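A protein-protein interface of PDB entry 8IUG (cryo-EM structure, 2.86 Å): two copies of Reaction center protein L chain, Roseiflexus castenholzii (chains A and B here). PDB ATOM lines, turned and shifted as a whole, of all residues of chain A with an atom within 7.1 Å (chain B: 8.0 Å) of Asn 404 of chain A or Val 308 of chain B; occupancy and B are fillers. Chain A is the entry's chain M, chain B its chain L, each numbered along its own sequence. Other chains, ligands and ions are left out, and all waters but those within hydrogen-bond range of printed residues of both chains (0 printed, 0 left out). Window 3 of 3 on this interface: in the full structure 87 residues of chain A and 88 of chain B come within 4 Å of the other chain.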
ATOM      1  N   GLY A 398      -3.660  -0.099 -13.315  1.00  0.00           N
ATOM      2  CA  GLY A 398      -4.754   0.688 -12.775  1.00  0.00           C
ATOM      3  C   GLY A 398      -4.393   2.145 -12.573  1.00  0.00           C
ATOM      4  O   GLY A 398      -5.203   3.034 -12.832  1.00  0.00           O
ATOM      5  N   VAL A 401      -4.392   3.927 -15.995  1.00  0.00           N
ATOM      6  CA  VAL A 401      -5.732   4.155 -16.529  1.00  0.00           C
ATOM      7  C   VAL A 401      -6.447   5.280 -15.786  1.00  0.00           C
ATOM      8  O   VAL A 401      -7.247   6.014 -16.376  1.00  0.00           O
ATOM      9  CB  VAL A 401      -6.526   2.836 -16.502  1.00  0.00           C
ATOM     10  CG1 VAL A 401      -7.938   3.058 -16.040  1.00  0.00           C
ATOM     11  CG2 VAL A 401      -6.515   2.206 -17.872  1.00  0.00           C
ATOM     12  N   GLY A 402      -6.167   5.451 -14.506  1.00  0.00           N
ATOM     13  CA  GLY A 402      -6.842   6.426 -13.686  1.00  0.00           C
ATOM     14  C   GLY A 402      -7.790   5.849 -12.660  1.00  0.00           C
ATOM     15  O   GLY A 402      -8.647   6.586 -12.161  1.00  0.00           O
ATOM     16  N   TRP A 403      -7.657   4.564 -12.325  1.00  0.00           N
ATOM     17  CA  TRP A 403      -8.551   3.855 -11.408  1.00  0.00           C
ATOM     18  C   TRP A 403      -9.983   3.805 -11.933  1.00  0.00           C
ATOM     19  O   TRP A 403     -10.938   3.857 -11.159  1.00  0.00           O
ATOM     20  CB  TRP A 403      -8.514   4.462  -9.998  1.00  0.00           C
ATOM     21  CG  TRP A 403      -7.126   4.711  -9.475  1.00  0.00           C
ATOM     22  CD1 TRP A 403      -6.543   5.918  -9.254  1.00  0.00           C
ATOM     23  CD2 TRP A 403      -6.155   3.726  -9.116  1.00  0.00           C
ATOM     24  NE1 TRP A 403      -5.269   5.751  -8.780  1.00  0.00           N
ATOM     25  CE2 TRP A 403      -5.006   4.413  -8.686  1.00  0.00           C
ATOM     26  CE3 TRP A 403      -6.145   2.330  -9.115  1.00  0.00           C
ATOM     27  CZ2 TRP A 403      -3.858   3.751  -8.263  1.00  0.00           C
ATOM     28  CZ3 TRP A 403      -5.006   1.677  -8.694  1.00  0.00           C
ATOM     29  CH2 TRP A 403      -3.879   2.387  -8.272  1.00  0.00           C
ATOM     30  N   ASN A 404     -10.145   3.695 -13.250  1.00  0.00           N
ATOM     31  CA  ASN A 404     -11.454   3.570 -13.882  1.00  0.00           C
ATOM     32  C   ASN A 404     -11.620   2.151 -14.405  1.00  0.00           C
ATOM     33  O   ASN A 404     -10.902   1.756 -15.336  1.00  0.00           O
ATOM     34  CB  ASN A 404     -11.598   4.581 -15.020  1.00  0.00           C
ATOM     35  CG  ASN A 404     -13.039   4.788 -15.449  1.00  0.00           C
ATOM     36  OD1 ASN A 404     -13.893   3.935 -15.240  1.00  0.00           O
ATOM     37  ND2 ASN A 404     -13.310   5.930 -16.059  1.00  0.00           N
ATOM     38  N   PRO A 405     -12.532   1.348 -13.847  1.00  0.00           N
ATOM     39  CA  PRO A 405     -12.621  -0.063 -14.260  1.00  0.00           C
ATOM     40  C   PRO A 405     -13.025  -0.273 -15.709  1.00  0.00           C
ATOM     41  O   PRO A 405     -12.582  -1.247 -16.329  1.00  0.00           O
ATOM     42  CB  PRO A 405     -13.671  -0.636 -13.299  1.00  0.00           C
ATOM     43  CG  PRO A 405     -13.752   0.325 -12.187  1.00  0.00           C
ATOM     44  CD  PRO A 405     -13.487   1.659 -12.777  1.00  0.00           C
ATOM     45  N   ILE A 406     -13.866   0.599 -16.265  1.00  0.00           N
ATOM     46  CA  ILE A 406     -14.332   0.412 -17.635  1.00  0.00           C
ATOM     47  C   ILE A 406     -13.216   0.705 -18.631  1.00  0.00           C
ATOM     48  O   ILE A 406     -13.023  -0.036 -19.602  1.00  0.00           O
ATOM     49  CB  ILE A 406     -15.577   1.277 -17.888  1.00  0.00           C
ATOM     50  CG1 ILE A 406     -16.578   1.103 -16.747  1.00  0.00           C
ATOM     51  CG2 ILE A 406     -16.226   0.901 -19.203  1.00  0.00           C
ATOM     52  CD1 ILE A 406     -17.843   1.887 -16.921  1.00  0.00           C
ATOM     53  N   ILE A 407     -12.464   1.786 -18.412  1.00  0.00           N
ATOM     54  CA  ILE A 407     -11.289   2.056 -19.236  1.00  0.00           C
ATOM     55  C   ILE A 407     -10.247   0.966 -19.038  1.00  0.00           C
ATOM     56  O   ILE A 407      -9.513   0.618 -19.969  1.00  0.00           O
ATOM     57  CB  ILE A 407     -10.716   3.450 -18.915  1.00  0.00           C
ATOM     58  CG1 ILE A 407     -11.772   4.528 -19.117  1.00  0.00           C
ATOM     59  CG2 ILE A 407      -9.509   3.752 -19.774  1.00  0.00           C
ATOM     60  CD1 ILE A 407     -11.239   5.918 -18.959  1.00  0.00           C
ATOM     61  N   TYR A 408     -10.159   0.420 -17.826  1.00  0.00           N
ATOM     62  CA  TYR A 408      -9.266  -0.702 -17.564  1.00  0.00           C
ATOM     63  C   TYR A 408      -9.614  -1.892 -18.447  1.00  0.00           C
ATOM     64  O   TYR A 408      -8.732  -2.509 -19.054  1.00  0.00           O
ATOM     65  CB  TYR A 408      -9.361  -1.081 -16.086  1.00  0.00           C
ATOM     66  CG  TYR A 408      -8.241  -1.940 -15.554  1.00  0.00           C
ATOM     67  CD1 TYR A 408      -8.198  -3.301 -15.805  1.00  0.00           C
ATOM     68  CD2 TYR A 408      -7.246  -1.392 -14.767  1.00  0.00           C
ATOM     69  CE1 TYR A 408      -7.184  -4.079 -15.307  1.00  0.00           C
ATOM     70  CE2 TYR A 408      -6.236  -2.166 -14.266  1.00  0.00           C
ATOM     71  CZ  TYR A 408      -6.209  -3.504 -14.538  1.00  0.00           C
ATOM     72  OH  TYR A 408      -5.196  -4.271 -14.032  1.00  0.00           O
ATOM     73  N   LEU A 409     -10.901  -2.231 -18.528  1.00  0.00           N
ATOM     74  CA  LEU A 409     -11.320  -3.356 -19.359  1.00  0.00           C
ATOM     75  C   LEU A 409     -11.128  -3.060 -20.842  1.00  0.00           C
ATOM     76  O   LEU A 409     -10.755  -3.951 -21.612  1.00  0.00           O
ATOM     77  CB  LEU A 409     -12.776  -3.708 -19.072  1.00  0.00           C
ATOM     78  CG  LEU A 409     -13.099  -4.349 -17.725  1.00  0.00           C
ATOM     79  CD1 LEU A 409     -14.589  -4.563 -17.599  1.00  0.00           C
ATOM     80  CD2 LEU A 409     -12.360  -5.659 -17.559  1.00  0.00           C
ATOM     81  N   ARG A 410     -11.405  -1.826 -21.266  1.00  0.00           N
ATOM     82  CA  ARG A 410     -11.258  -1.480 -22.676  1.00  0.00           C
ATOM     83  C   ARG A 410      -9.805  -1.540 -23.123  1.00  0.00           C
ATOM     84  O   ARG A 410      -9.505  -2.053 -24.206  1.00  0.00           O
ATOM     85  CB  ARG A 410     -11.841  -0.092 -22.941  1.00  0.00           C
ATOM     86  CG  ARG A 410     -11.252   0.583 -24.159  1.00  0.00           C
ATOM     87  CD  ARG A 410     -12.151   1.643 -24.753  1.00  0.00           C
ATOM     88  NE  ARG A 410     -12.475   2.727 -23.838  1.00  0.00           N
ATOM     89  CZ  ARG A 410     -11.690   3.766 -23.589  1.00  0.00           C
ATOM     90  NH1 ARG A 410     -10.473   3.845 -24.088  1.00  0.00           N
ATOM     91  NH2 ARG A 410     -12.141   4.749 -22.819  1.00  0.00           N
ATOM     92  N   ASP B 300     -12.656   0.144 -29.813  1.00  0.00           N
ATOM     93  CA  ASP B 300     -12.934   1.274 -28.938  1.00  0.00           C
ATOM     94  C   ASP B 300     -14.251   1.963 -29.257  1.00  0.00           C
ATOM     95  O   ASP B 300     -14.612   2.913 -28.557  1.00  0.00           O
ATOM     96  CB  ASP B 300     -11.794   2.293 -29.005  1.00  0.00           C
ATOM     97  CG  ASP B 300     -10.616   1.911 -28.136  1.00  0.00           C
ATOM     98  OD1 ASP B 300     -10.650   0.821 -27.538  1.00  0.00           O
ATOM     99  OD2 ASP B 300      -9.654   2.698 -28.043  1.00  0.00           O
ATOM    100  N   PRO B 303     -20.510   0.194 -27.946  1.00  0.00           N
ATOM    101  CA  PRO B 303     -21.277   1.067 -27.043  1.00  0.00           C
ATOM    102  C   PRO B 303     -21.044   0.809 -25.568  1.00  0.00           C
ATOM    103  O   PRO B 303     -21.430   1.644 -24.744  1.00  0.00           O
ATOM    104  CB  PRO B 303     -22.732   0.777 -27.430  1.00  0.00           C
ATOM    105  CG  PRO B 303     -22.656   0.204 -28.792  1.00  0.00           C
ATOM    106  CD  PRO B 303     -21.391  -0.575 -28.837  1.00  0.00           C
ATOM    107  N   ILE B 304     -20.439  -0.321 -25.205  1.00  0.00           N
ATOM    108  CA  ILE B 304     -20.268  -0.660 -23.798  1.00  0.00           C
ATOM    109  C   ILE B 304     -19.265   0.260 -23.116  1.00  0.00           C
ATOM    110  O   ILE B 304     -19.361   0.497 -21.908  1.00  0.00           O
ATOM    111  CB  ILE B 304     -19.863  -2.137 -23.658  1.00  0.00           C
ATOM    112  CG1 ILE B 304     -18.841  -2.513 -24.729  1.00  0.00           C
ATOM    113  CG2 ILE B 304     -21.084  -3.021 -23.760  1.00  0.00           C
ATOM    114  CD1 ILE B 304     -18.368  -3.929 -24.645  1.00  0.00           C
ATOM    115  N   TRP B 305     -18.280   0.778 -23.852  1.00  0.00           N
ATOM    116  CA  TRP B 305     -17.244   1.575 -23.210  1.00  0.00           C
ATOM    117  C   TRP B 305     -16.804   2.802 -23.999  1.00  0.00           C
ATOM    118  O   TRP B 305     -15.826   3.444 -23.603  1.00  0.00           O
ATOM    119  CB  TRP B 305     -16.026   0.701 -22.893  1.00  0.00           C
ATOM    120  CG  TRP B 305     -15.555  -0.176 -24.008  1.00  0.00           C
ATOM    121  CD1 TRP B 305     -15.501   0.130 -25.332  1.00  0.00           C
ATOM    122  CD2 TRP B 305     -15.069  -1.513 -23.887  1.00  0.00           C
ATOM    123  NE1 TRP B 305     -15.005  -0.932 -26.044  1.00  0.00           N
ATOM    124  CE2 TRP B 305     -14.735  -1.955 -25.176  1.00  0.00           C
ATOM    125  CE3 TRP B 305     -14.885  -2.381 -22.808  1.00  0.00           C
ATOM    126  CZ2 TRP B 305     -14.224  -3.222 -25.416  1.00  0.00           C
ATOM    127  CZ3 TRP B 305     -14.381  -3.637 -23.050  1.00  0.00           C
ATOM    128  CH2 TRP B 305     -14.056  -4.048 -24.342  1.00  0.00           C
ATOM    129  N   ASN B 306     -17.476   3.160 -25.086  1.00  0.00           N
ATOM    130  CA  ASN B 306     -17.171   4.420 -25.745  1.00  0.00           C
ATOM    131  C   ASN B 306     -17.797   5.573 -24.972  1.00  0.00           C
ATOM    132  O   ASN B 306     -18.858   5.437 -24.364  1.00  0.00           O
ATOM    133  CB  ASN B 306     -17.660   4.417 -27.196  1.00  0.00           C
ATOM    134  CG  ASN B 306     -19.162   4.295 -27.316  1.00  0.00           C
ATOM    135  OD1 ASN B 306     -19.841   3.899 -26.379  1.00  0.00           O
ATOM    136  ND2 ASN B 306     -19.687   4.625 -28.484  1.00  0.00           N
ATOM    137  N   GLY B 307     -17.126   6.715 -24.986  1.00  0.00           N
ATOM    138  CA  GLY B 307     -17.646   7.854 -24.253  1.00  0.00           C
ATOM    139  C   GLY B 307     -17.665   7.707 -22.748  1.00  0.00           C
ATOM    140  O   GLY B 307     -18.660   8.063 -22.109  1.00  0.00           O
ATOM    141  N   VAL B 308     -16.583   7.205 -22.160  1.00  0.00           N
ATOM    142  CA  VAL B 308     -16.470   7.106 -20.708  1.00  0.00           C
ATOM    143  C   VAL B 308     -15.191   7.728 -20.166  1.00  0.00           C
ATOM    144  O   VAL B 308     -15.061   7.859 -18.940  1.00  0.00           O
ATOM    145  CB  VAL B 308     -16.598   5.642 -20.228  1.00  0.00           C
ATOM    146  CG1 VAL B 308     -15.251   4.949 -20.225  1.00  0.00           C
ATOM    147  CG2 VAL B 308     -17.249   5.578 -18.863  1.00  0.00           C
ATOM    148  N   GLY B 309     -14.255   8.146 -21.018  1.00  0.00           N
ATOM    149  CA  GLY B 309     -13.008   8.729 -20.578  1.00  0.00           C
ATOM    150  C   GLY B 309     -12.937  10.236 -20.798  1.00  0.00           C
ATOM    151  O   GLY B 309     -13.819  10.855 -21.386  1.00  0.00           O
ATOM    152  N   GLN B 310     -11.848  10.817 -20.301  1.00  0.00           N
ATOM    153  CA  GLN B 310     -11.527  12.229 -20.456  1.00  0.00           C
ATOM    154  C   GLN B 310     -10.329  12.380 -21.386  1.00  0.00           C
ATOM    155  O   GLN B 310      -9.869  11.411 -21.992  1.00  0.00           O
ATOM    156  CB  GLN B 310     -11.272  12.869 -19.093  1.00  0.00           C
ATOM    157  CG  GLN B 310     -12.529  13.104 -18.279  1.00  0.00           C
ATOM    158  CD  GLN B 310     -13.443  14.122 -18.916  1.00  0.00           C
ATOM    159  OE1 GLN B 310     -12.985  15.048 -19.581  1.00  0.00           O
ATOM    160  NE2 GLN B 310     -14.743  13.953 -18.722  1.00  0.00           N
ATOM    161  N   LEU B 313      -7.671  10.029 -22.629  1.00  0.00           N
ATOM    162  CA  LEU B 313      -8.253   8.751 -22.238  1.00  0.00           C
ATOM    163  C   LEU B 313      -9.595   8.527 -22.923  1.00  0.00           C
ATOM    164  O   LEU B 313     -10.364   7.656 -22.510  1.00  0.00           O
ATOM    165  CB  LEU B 313      -8.408   8.661 -20.718  1.00  0.00           C
ATOM    166  CG  LEU B 313      -7.176   8.299 -19.885  1.00  0.00           C
ATOM    167  CD1 LEU B 313      -7.441   8.533 -18.421  1.00  0.00           C
ATOM    168  CD2 LEU B 313      -6.778   6.859 -20.111  1.00  0.00           C
ATOM    169  N   VAL B 314      -9.888   9.307 -23.961  1.00  0.00           N
ATOM    170  CA  VAL B 314     -11.136   9.226 -24.708  1.00  0.00           C
ATOM    171  C   VAL B 314     -11.128   8.001 -25.612  1.00  0.00           C
ATOM    172  O   VAL B 314     -10.105   7.320 -25.741  1.00  0.00           O
ATOM    173  CB  VAL B 314     -11.374  10.502 -25.535  1.00  0.00           C
ATOM    174  CG1 VAL B 314     -11.556  11.694 -24.634  1.00  0.00           C
ATOM    175  CG2 VAL B 314     -10.226  10.727 -26.491  1.00  0.00           C
ATOM    176  N   ALA B 315     -12.284   7.705 -26.205  1.00  0.00           N
ATOM    177  CA  ALA B 315     -12.471   6.633 -27.184  1.00  0.00           C
ATOM    178  C   ALA B 315     -12.424   5.274 -26.526  1.00  0.00           C
ATOM    179  O   ALA B 315     -13.403   4.533 -26.570  1.00  0.00           O
ATOM    180  CB  ALA B 315     -11.439   6.717 -28.301  1.00  0.00           C
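The backbone carbonyl oxygen of Trp 305 of chain B sits at hydrogen-bond distance from the guanidinium group of Arg 410 of chain A (3.4 Å).
The guanidinium group (NH2) of Arg 410 of chain A sits at hydrogen-bond distance from the backbone carbonyl oxygen (O) of Leu 313 of chain B, 3.4 Å away.
O of Ala 315 of chain B is in hydrogen-bond range of NE of Arg 410 of chain A (3.4 Å).
OD1 of Asn 404 of chain A lies close to N of Ile 406 of chain A.
CD1 of Leu 313 of chain B touches O of Val 401 of chain A (3.3 Å).
O of Val 308 of chain B touches ND2 of Asn 404 of chain A, 3.9 Å away.
Trp 305 of chain B touches Ile 406 of chain A (CB to CG2, 3.7 Å).
CG1 of Val 308 of chain B touches CG1 of Ile 407 of chain A, at 3.7 Å.
Ile 407 of chain A touches Gly 309 of chain B (CD1 to CA, 3.7 Å).
Trp 305 of chain B touches Leu 409 of chain A.
Arg 410 of chain A touches Asp 300 of chain B (CD to OD1, 3.3 Å).
Arg 410 of chain A touches Val 314 of chain B.
Asn 404 of chain A touches just one residue of chain B: Val 308 (3.9 Å).
Of chain A, only Asn 404 and Ile 407 come within 4 Å of Val 308 of chain B.
No residue of chain B comes within 4 Å of Pro 405 of chain A.
No residue of chain A comes within 4 Å of Gly 307 of chain B.
Of the printed residues of chain B, Ile 407 of chain A touches Val 308 and Gly 309.
Of the printed residues of chain B, Arg 410 of chain A touches Asp 300 (3.3 Å), Trp 305 (3.4 Å), Leu 313 (3.4 Å), Val 314 (3.9 Å) and Ala 315 (3.4 Å).
Of the printed residues of chain A, Trp 305 of chain B touches Ile 406, Leu 409 and Arg 410.
Printed residues of chain B within 4 Å of Leu 409 of chain A: Trp 305.
Of the printed residues of chain A, Val 314 of chain B touches Arg 410 (3.9 Å).
Gly 402 of chain A touches none of the printed residues of chain B.
Of the 11 printed residues of chain A, 6 touch a printed residue of chain B.
Hydrophobic or aromatic side chains of chain A within 4 Å of the printed part of chain B: Ile 406 and Ile 407.
Printed residues of chain B that touch a printed residue of chain A: Asp 300, Trp 305, Val 308, Gly 309, Leu 313, Val 314 and Ala 315.
Among the printed residues, 11 pairs touch across the chains.
Among the printed residues, no Asp or Glu carboxylate lies within 4 Å of a Lys or Arg side-chain nitrogen of the other chain.
No position is printed for both chains.
Of the 11 pairs that touch across the chains among the printed residues, none has its exchanged pair printed and touching as well.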
